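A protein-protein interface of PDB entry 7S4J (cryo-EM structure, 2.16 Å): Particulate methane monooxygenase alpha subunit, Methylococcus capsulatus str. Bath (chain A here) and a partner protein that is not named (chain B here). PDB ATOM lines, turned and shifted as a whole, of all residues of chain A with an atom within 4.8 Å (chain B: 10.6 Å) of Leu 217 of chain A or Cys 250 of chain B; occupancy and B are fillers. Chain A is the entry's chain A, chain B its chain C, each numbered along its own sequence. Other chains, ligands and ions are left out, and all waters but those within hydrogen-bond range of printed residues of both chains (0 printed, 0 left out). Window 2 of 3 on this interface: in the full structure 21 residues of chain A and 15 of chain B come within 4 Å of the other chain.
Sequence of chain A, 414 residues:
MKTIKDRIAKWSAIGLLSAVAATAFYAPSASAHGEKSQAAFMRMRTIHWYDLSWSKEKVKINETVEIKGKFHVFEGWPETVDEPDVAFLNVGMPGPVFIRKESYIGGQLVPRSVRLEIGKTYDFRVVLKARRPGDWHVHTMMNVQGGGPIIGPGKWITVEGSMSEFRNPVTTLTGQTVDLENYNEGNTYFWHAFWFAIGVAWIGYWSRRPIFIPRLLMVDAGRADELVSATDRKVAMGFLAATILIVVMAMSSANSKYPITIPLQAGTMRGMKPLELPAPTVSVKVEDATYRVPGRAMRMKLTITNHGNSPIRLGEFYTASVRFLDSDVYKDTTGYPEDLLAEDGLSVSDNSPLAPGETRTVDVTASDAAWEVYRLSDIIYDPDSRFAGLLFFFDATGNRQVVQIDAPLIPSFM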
ATOM      1  N   ILE A 213       5.404  24.576 -15.375  1.00  0.00           N
ATOM      2  CA  ILE A 213       4.781  23.391 -15.968  1.00  0.00           C
ATOM      3  C   ILE A 213       5.696  22.172 -15.886  1.00  0.00           C
ATOM      4  O   ILE A 213       5.227  21.100 -15.476  1.00  0.00           O
ATOM      5  CB  ILE A 213       4.330  23.661 -17.413  1.00  0.00           C
ATOM      6  CG1 ILE A 213       3.140  24.624 -17.421  1.00  0.00           C
ATOM      7  CG2 ILE A 213       3.958  22.364 -18.107  1.00  0.00           C
ATOM      8  CD1 ILE A 213       2.401  24.682 -18.737  1.00  0.00           C
ATOM      9  N   PRO A 214       6.978  22.251 -16.269  1.00  0.00           N
ATOM     10  CA  PRO A 214       7.834  21.064 -16.096  1.00  0.00           C
ATOM     11  C   PRO A 214       7.973  20.624 -14.650  1.00  0.00           C
ATOM     12  O   PRO A 214       7.983  19.420 -14.380  1.00  0.00           O
ATOM     13  CB  PRO A 214       9.175  21.508 -16.696  1.00  0.00           C
ATOM     14  CG  PRO A 214       9.140  22.971 -16.666  1.00  0.00           C
ATOM     15  CD  PRO A 214       7.722  23.354 -16.901  1.00  0.00           C
ATOM     16  N   ARG A 215       8.056  21.561 -13.703  1.00  0.00           N
ATOM     17  CA  ARG A 215       8.170  21.172 -12.301  1.00  0.00           C
ATOM     18  C   ARG A 215       6.878  20.545 -11.797  1.00  0.00           C
ATOM     19  O   ARG A 215       6.910  19.570 -11.037  1.00  0.00           O
ATOM     20  CB  ARG A 215       8.559  22.379 -11.450  1.00  0.00           C
ATOM     21  CG  ARG A 215      10.007  22.787 -11.619  1.00  0.00           C
ATOM     22  CD  ARG A 215      10.375  23.971 -10.749  1.00  0.00           C
ATOM     23  NE  ARG A 215      10.716  23.571  -9.392  1.00  0.00           N
ATOM     24  CZ  ARG A 215      11.942  23.271  -8.990  1.00  0.00           C
ATOM     25  NH1 ARG A 215      12.963  23.282  -9.827  1.00  0.00           N
ATOM     26  NH2 ARG A 215      12.146  22.947  -7.718  1.00  0.00           N
ATOM     27  N   LEU A 216       5.733  21.084 -12.215  1.00  0.00           N
ATOM     28  CA  LEU A 216       4.452  20.486 -11.862  1.00  0.00           C
ATOM     29  C   LEU A 216       4.345  19.070 -12.407  1.00  0.00           C
ATOM     30  O   LEU A 216       3.914  18.153 -11.697  1.00  0.00           O
ATOM     31  CB  LEU A 216       3.315  21.352 -12.402  1.00  0.00           C
ATOM     32  CG  LEU A 216       1.885  20.829 -12.294  1.00  0.00           C
ATOM     33  CD1 LEU A 216       1.405  20.863 -10.860  1.00  0.00           C
ATOM     34  CD2 LEU A 216       0.967  21.634 -13.189  1.00  0.00           C
ATOM     35  N   LEU A 217       4.749  18.870 -13.662  1.00  0.00           N
ATOM     36  CA  LEU A 217       4.677  17.541 -14.257  1.00  0.00           C
ATOM     37  C   LEU A 217       5.648  16.579 -13.586  1.00  0.00           C
ATOM     38  O   LEU A 217       5.343  15.394 -13.437  1.00  0.00           O
ATOM     39  CB  LEU A 217       4.947  17.618 -15.757  1.00  0.00           C
ATOM     40  CG  LEU A 217       3.904  18.378 -16.578  1.00  0.00           C
ATOM     41  CD1 LEU A 217       4.357  18.525 -18.017  1.00  0.00           C
ATOM     42  CD2 LEU A 217       2.543  17.715 -16.496  1.00  0.00           C
ATOM     43  N   MET A 218       6.826  17.059 -13.189  1.00  0.00           N
ATOM     44  CA  MET A 218       7.774  16.188 -12.504  1.00  0.00           C
ATOM     45  C   MET A 218       7.278  15.802 -11.117  1.00  0.00           C
ATOM     46  O   MET A 218       7.448  14.654 -10.693  1.00  0.00           O
ATOM     47  CB  MET A 218       9.143  16.858 -12.417  1.00  0.00           C
ATOM     48  CG  MET A 218       9.853  16.977 -13.748  1.00  0.00           C
ATOM     49  SD  MET A 218      11.015  15.633 -14.043  1.00  0.00           S
ATOM     50  CE  MET A 218      12.028  15.726 -12.569  1.00  0.00           C
ATOM     51  N   VAL A 219       6.669  16.741 -10.390  1.00  0.00           N
ATOM     52  CA  VAL A 219       6.145  16.417  -9.067  1.00  0.00           C
ATOM     53  C   VAL A 219       4.961  15.467  -9.184  1.00  0.00           C
ATOM     54  O   VAL A 219       4.797  14.555  -8.364  1.00  0.00           O
ATOM     55  CB  VAL A 219       5.776  17.701  -8.300  1.00  0.00           C
ATOM     56  CG1 VAL A 219       5.062  17.365  -7.010  1.00  0.00           C
ATOM     57  CG2 VAL A 219       7.011  18.515  -8.007  1.00  0.00           C
ATOM     58  N   ASP A 220       4.124  15.653 -10.205  1.00  0.00           N
ATOM     59  CA  ASP A 220       2.978  14.766 -10.410  1.00  0.00           C
ATOM     60  C   ASP A 220       3.430  13.369 -10.824  1.00  0.00           C
ATOM     61  O   ASP A 220       3.095  12.376 -10.173  1.00  0.00           O
ATOM     62  CB  ASP A 220       2.038  15.365 -11.461  1.00  0.00           C
ATOM     63  CG  ASP A 220       1.254  16.547 -10.936  1.00  0.00           C
ATOM     64  OD1 ASP A 220       1.407  16.881  -9.742  1.00  0.00           O
ATOM     65  OD2 ASP A 220       0.489  17.147 -11.718  1.00  0.00           O
ATOM     66  N   ALA A 221       4.194  13.281 -11.910  1.00  0.00           N
ATOM     67  CA  ALA A 221       4.622  12.005 -12.462  1.00  0.00           C
ATOM     68  C   ALA A 221       5.701  11.384 -11.594  1.00  0.00           C
ATOM     69  O   ALA A 221       6.893  11.627 -11.801  1.00  0.00           O
ATOM     70  CB  ALA A 221       5.136  12.181 -13.891  1.00  0.00           C
ATOM     71  N   THR B 234      -3.138  26.163 -11.483  1.00  0.00           N
ATOM     72  CA  THR B 234      -2.823  24.771 -11.785  1.00  0.00           C
ATOM     73  C   THR B 234      -3.841  24.179 -12.753  1.00  0.00           C
ATOM     74  O   THR B 234      -3.481  23.356 -13.604  1.00  0.00           O
ATOM     75  CB  THR B 234      -2.709  23.934 -10.508  1.00  0.00           C
ATOM     76  OG1 THR B 234      -2.572  22.551 -10.852  1.00  0.00           O
ATOM     77  CG2 THR B 234      -3.906  24.100  -9.635  1.00  0.00           C
ATOM     78  N   GLN B 235      -5.102  24.618 -12.677  1.00  0.00           N
ATOM     79  CA  GLN B 235      -6.075  24.202 -13.682  1.00  0.00           C
ATOM     80  C   GLN B 235      -5.692  24.698 -15.073  1.00  0.00           C
ATOM     81  O   GLN B 235      -5.790  23.949 -16.050  1.00  0.00           O
ATOM     82  CB  GLN B 235      -7.465  24.696 -13.292  1.00  0.00           C
ATOM     83  CG  GLN B 235      -8.262  23.685 -12.502  1.00  0.00           C
ATOM     84  CD  GLN B 235      -9.618  24.204 -12.097  1.00  0.00           C
ATOM     85  OE1 GLN B 235      -9.960  25.352 -12.365  1.00  0.00           O
ATOM     86  NE2 GLN B 235     -10.403  23.359 -11.445  1.00  0.00           N
ATOM     87  N   THR B 236      -5.251  25.955 -15.188  1.00  0.00           N
ATOM     88  CA  THR B 236      -4.823  26.458 -16.492  1.00  0.00           C
ATOM     89  C   THR B 236      -3.562  25.761 -16.981  1.00  0.00           C
ATOM     90  O   THR B 236      -3.397  25.573 -18.185  1.00  0.00           O
ATOM     91  CB  THR B 236      -4.586  27.971 -16.475  1.00  0.00           C
ATOM     92  OG1 THR B 236      -3.319  28.259 -15.875  1.00  0.00           O
ATOM     93  CG2 THR B 236      -5.683  28.698 -15.752  1.00  0.00           C
ATOM     94  N   PHE B 237      -2.661  25.387 -16.075  1.00  0.00           N
ATOM     95  CA  PHE B 237      -1.484  24.625 -16.476  1.00  0.00           C
ATOM     96  C   PHE B 237      -1.885  23.271 -17.046  1.00  0.00           C
ATOM     97  O   PHE B 237      -1.357  22.838 -18.075  1.00  0.00           O
ATOM     98  CB  PHE B 237      -0.538  24.450 -15.290  1.00  0.00           C
ATOM     99  CG  PHE B 237       0.170  25.708 -14.889  1.00  0.00           C
ATOM    100  CD1 PHE B 237       0.393  26.716 -15.807  1.00  0.00           C
ATOM    101  CD2 PHE B 237       0.602  25.885 -13.589  1.00  0.00           C
ATOM    102  CE1 PHE B 237       1.037  27.872 -15.435  1.00  0.00           C
ATOM    103  CE2 PHE B 237       1.246  27.040 -13.214  1.00  0.00           C
ATOM    104  CZ  PHE B 237       1.463  28.033 -14.137  1.00  0.00           C
ATOM    105  N   TYR B 238      -2.823  22.589 -16.385  1.00  0.00           N
ATOM    106  CA  TYR B 238      -3.307  21.316 -16.910  1.00  0.00           C
ATOM    107  C   TYR B 238      -4.002  21.501 -18.252  1.00  0.00           C
ATOM    108  O   TYR B 238      -3.838  20.681 -19.162  1.00  0.00           O
ATOM    109  CB  TYR B 238      -4.245  20.653 -15.905  1.00  0.00           C
ATOM    110  CG  TYR B 238      -3.519  20.004 -14.754  1.00  0.00           C
ATOM    111  CD1 TYR B 238      -2.349  19.294 -14.963  1.00  0.00           C
ATOM    112  CD2 TYR B 238      -4.001  20.105 -13.460  1.00  0.00           C
ATOM    113  CE1 TYR B 238      -1.681  18.701 -13.916  1.00  0.00           C
ATOM    114  CE2 TYR B 238      -3.340  19.516 -12.408  1.00  0.00           C
ATOM    115  CZ  TYR B 238      -2.181  18.815 -12.642  1.00  0.00           C
ATOM    116  OH  TYR B 238      -1.519  18.225 -11.593  1.00  0.00           O
ATOM    117  N   SER B 239      -4.786  22.570 -18.393  1.00  0.00           N
ATOM    118  CA  SER B 239      -5.427  22.860 -19.672  1.00  0.00           C
ATOM    119  C   SER B 239      -4.397  23.120 -20.761  1.00  0.00           C
ATOM    120  O   SER B 239      -4.590  22.707 -21.909  1.00  0.00           O
ATOM    121  CB  SER B 239      -6.366  24.056 -19.525  1.00  0.00           C
ATOM    122  OG  SER B 239      -6.431  24.811 -20.718  1.00  0.00           O
ATOM    123  N   PHE B 240      -3.310  23.808 -20.419  1.00  0.00           N
ATOM    124  CA  PHE B 240      -2.207  24.007 -21.350  1.00  0.00           C
ATOM    125  C   PHE B 240      -1.585  22.679 -21.754  1.00  0.00           C
ATOM    126  O   PHE B 240      -1.280  22.460 -22.932  1.00  0.00           O
ATOM    127  CB  PHE B 240      -1.153  24.902 -20.704  1.00  0.00           C
ATOM    128  CG  PHE B 240      -1.168  26.317 -21.188  1.00  0.00           C
ATOM    129  CD1 PHE B 240      -0.729  26.637 -22.455  1.00  0.00           C
ATOM    130  CD2 PHE B 240      -1.614  27.334 -20.362  1.00  0.00           C
ATOM    131  CE1 PHE B 240      -0.737  27.942 -22.892  1.00  0.00           C
ATOM    132  CE2 PHE B 240      -1.625  28.637 -20.794  1.00  0.00           C
ATOM    133  CZ  PHE B 240      -1.185  28.942 -22.059  1.00  0.00           C
ATOM    134  N   ALA B 241      -1.380  21.788 -20.792  1.00  0.00           N
ATOM    135  CA  ALA B 241      -0.746  20.493 -21.034  1.00  0.00           C
ATOM    136  C   ALA B 241      -1.771  19.396 -21.289  1.00  0.00           C
ATOM    137  O   ALA B 241      -1.710  18.321 -20.697  1.00  0.00           O
ATOM    138  CB  ALA B 241       0.152  20.134 -19.858  1.00  0.00           C
ATOM    139  N   GLN B 242      -2.722  19.638 -22.188  1.00  0.00           N
ATOM    140  CA  GLN B 242      -3.713  18.616 -22.548  1.00  0.00           C
ATOM    141  C   GLN B 242      -3.248  17.864 -23.789  1.00  0.00           C
ATOM    142  O   GLN B 242      -3.054  16.645 -23.755  1.00  0.00           O
ATOM    143  CB  GLN B 242      -5.085  19.258 -22.769  1.00  0.00           C
ATOM    144  CG  GLN B 242      -5.873  19.539 -21.501  1.00  0.00           C
ATOM    145  CD  GLN B 242      -6.521  18.299 -20.925  1.00  0.00           C
ATOM    146  OE1 GLN B 242      -5.842  17.363 -20.506  1.00  0.00           O
ATOM    147  NE2 GLN B 242      -7.849  18.285 -20.903  1.00  0.00           N
ATOM    148  N   GLY B 243      -3.073  18.584 -24.892  1.00  0.00           N
ATOM    149  CA  GLY B 243      -2.503  18.015 -26.094  1.00  0.00           C
ATOM    150  C   GLY B 243      -1.148  18.619 -26.383  1.00  0.00           C
ATOM    151  O   GLY B 243      -0.247  17.948 -26.897  1.00  0.00           O
ATOM    152  N   GLY B 244      -0.992  19.894 -26.036  1.00  0.00           N
ATOM    153  CA  GLY B 244       0.253  20.598 -26.261  1.00  0.00           C
ATOM    154  C   GLY B 244       1.195  20.540 -25.076  1.00  0.00           C
ATOM    155  O   GLY B 244       1.998  21.455 -24.865  1.00  0.00           O
ATOM    156  N   LEU B 245       1.099  19.467 -24.288  1.00  0.00           N
ATOM    157  CA  LEU B 245       2.016  19.284 -23.174  1.00  0.00           C
ATOM    158  C   LEU B 245       3.451  19.175 -23.648  1.00  0.00           C
ATOM    159  O   LEU B 245       4.368  19.519 -22.900  1.00  0.00           O
ATOM    160  CB  LEU B 245       1.617  18.044 -22.359  1.00  0.00           C
ATOM    161  CG  LEU B 245       2.536  17.404 -21.310  1.00  0.00           C
ATOM    162  CD1 LEU B 245       1.688  16.659 -20.287  1.00  0.00           C
ATOM    163  CD2 LEU B 245       3.550  16.443 -21.923  1.00  0.00           C
ATOM    164  N   GLY B 246       3.659  18.714 -24.878  1.00  0.00           N
ATOM    165  CA  GLY B 246       4.989  18.579 -25.425  1.00  0.00           C
ATOM    166  C   GLY B 246       4.940  18.103 -26.859  1.00  0.00           C
ATOM    167  O   GLY B 246       4.056  18.475 -27.634  1.00  0.00           O
ATOM    168  N   GLN B 247       5.894  17.244 -27.191  1.00  0.00           N
ATOM    169  CA  GLN B 247       6.786  16.715 -26.172  1.00  0.00           C
ATOM    170  C   GLN B 247       8.109  17.460 -26.117  1.00  0.00           C
ATOM    171  O   GLN B 247       8.463  18.183 -27.048  1.00  0.00           O
ATOM    172  CB  GLN B 247       7.014  15.218 -26.393  1.00  0.00           C
ATOM    173  CG  GLN B 247       5.800  14.353 -26.024  1.00  0.00           C
ATOM    174  CD  GLN B 247       5.161  14.731 -24.682  1.00  0.00           C
ATOM    175  OE1 GLN B 247       5.799  15.318 -23.806  1.00  0.00           O
ATOM    176  NE2 GLN B 247       3.880  14.416 -24.537  1.00  0.00           N
ATOM    177  N   SER B 248       8.854  17.170 -25.047  1.00  0.00           N
ATOM    178  CA  SER B 248       9.875  18.019 -24.444  1.00  0.00           C
ATOM    179  C   SER B 248       9.678  17.947 -22.941  1.00  0.00           C
ATOM    180  O   SER B 248      10.516  17.408 -22.211  1.00  0.00           O
ATOM    181  CB  SER B 248       9.786  19.473 -24.902  1.00  0.00           C
ATOM    182  OG  SER B 248      10.457  20.329 -23.997  1.00  0.00           O
ATOM    183  N   LEU B 249       8.575  18.522 -22.482  1.00  0.00           N
ATOM    184  CA  LEU B 249       8.144  18.372 -21.103  1.00  0.00           C
ATOM    185  C   LEU B 249       8.051  16.895 -20.750  1.00  0.00           C
ATOM    186  O   LEU B 249       7.502  16.099 -21.517  1.00  0.00           O
ATOM    187  CB  LEU B 249       6.788  19.054 -20.904  1.00  0.00           C
ATOM    188  CG  LEU B 249       6.624  20.582 -20.933  1.00  0.00           C
ATOM    189  CD1 LEU B 249       7.191  21.197 -19.680  1.00  0.00           C
ATOM    190  CD2 LEU B 249       7.208  21.250 -22.171  1.00  0.00           C
ATOM    191  N   CYS B 250       8.599  16.533 -19.593  1.00  0.00           N
ATOM    192  CA  CYS B 250       8.641  15.145 -19.135  1.00  0.00           C
ATOM    193  C   CYS B 250       9.389  14.254 -20.123  1.00  0.00           C
ATOM    194  O   CYS B 250       9.052  13.085 -20.321  1.00  0.00           O
ATOM    195  CB  CYS B 250       7.233  14.605 -18.877  1.00  0.00           C
ATOM    196  SG  CYS B 250       6.688  14.746 -17.164  1.00  0.00           S
ATOM    197  N   GLU B 251      10.423  14.818 -20.738  1.00  0.00           N
ATOM    198  CA  GLU B 251      11.298  14.052 -21.616  1.00  0.00           C
ATOM    199  C   GLU B 251      12.602  14.792 -21.891  1.00  0.00           C
ATOM    200  O   GLU B 251      13.620  14.529 -21.251  1.00  0.00           O
ATOM    201  CB  GLU B 251      10.594  13.737 -22.933  1.00  0.00           C
ATOM    202  CG  GLU B 251      10.965  14.657 -24.079  1.00  0.00           C
ATOM    203  CD  GLU B 251      10.424  14.163 -25.400  1.00  0.00           C
ATOM    204  OE1 GLU B 251       9.532  13.291 -25.381  1.00  0.00           O
ATOM    205  OE2 GLU B 251      10.887  14.639 -26.457  1.00  0.00           O
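Ile 213 of chain A touches Phe 237 of chain B.
CD1 of Leu 249 of chain B touches CG2 of Ile 213 of chain A (3.8 Å).
CD of Pro 214 of chain A touches CD1 of Leu 249 of chain B (3.6 Å).
CD2 of Leu 216 of chain A touches CB of Phe 237 of chain B (3.8 Å).
Leu 217 of chain A touches Leu 245 of chain B.
Leu 217 of chain A touches Leu 249 of chain B.
Cys 250 of chain B touches Leu 217 of chain A.
The side-chain hydroxyl (OH) of Tyr 238 of chain B sits close to the side-chain carboxylate (OD2) of Asp 220 of chain A, 2.3 Å away.
The backbone carbonyl oxygen (O) of Leu 249 of chain B lies close to the side-chain amide oxygen (OE1) of Gln 247 of chain B (3.0 Å).
Of the 9 printed residues of chain A, 5 touch a printed residue of chain B.
Hydrophobic or aromatic side chains of chain B within 4 Å of the printed part of chain A: Phe 237, Tyr 238, Leu 245 and Leu 249.
Along chain B the printed residues that touch a printed residue of chain A span positions 237 to 250.
Among the printed residues, no Asp or Glu carboxylate lies within 4 Å of a Lys or Arg side-chain nitrogen of the other chain.
Of chain B, only Phe 237 and Leu 249 come within 4 Å of Ile 213 of chain A.
Of the printed residues of chain B, Pro 214 of chain A touches Leu 249 (3.6 Å).
Leu 217 of chain A touches just these residues of chain B: Leu 245, Leu 249 and Cys 250.
No residue of chain B comes within 4 Å of Met 218 of chain A.
No residue of chain B comes within 4 Å of Ala 221 of chain A.
Printed residues of chain A within 4 Å of Leu 245 of chain B: Leu 217 (3.9 Å).
Cys 250 of chain B touches just one residue of chain A: Leu 217 (3.6 Å).
The nearest residue of chain B that does not touch Leu 217 of chain A is Ala 241 of chain B (4.8 Å).
The nearest printed residue of chain B that does not touch Pro 214 of chain A is Cys 250 of chain B (5.6 Å).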
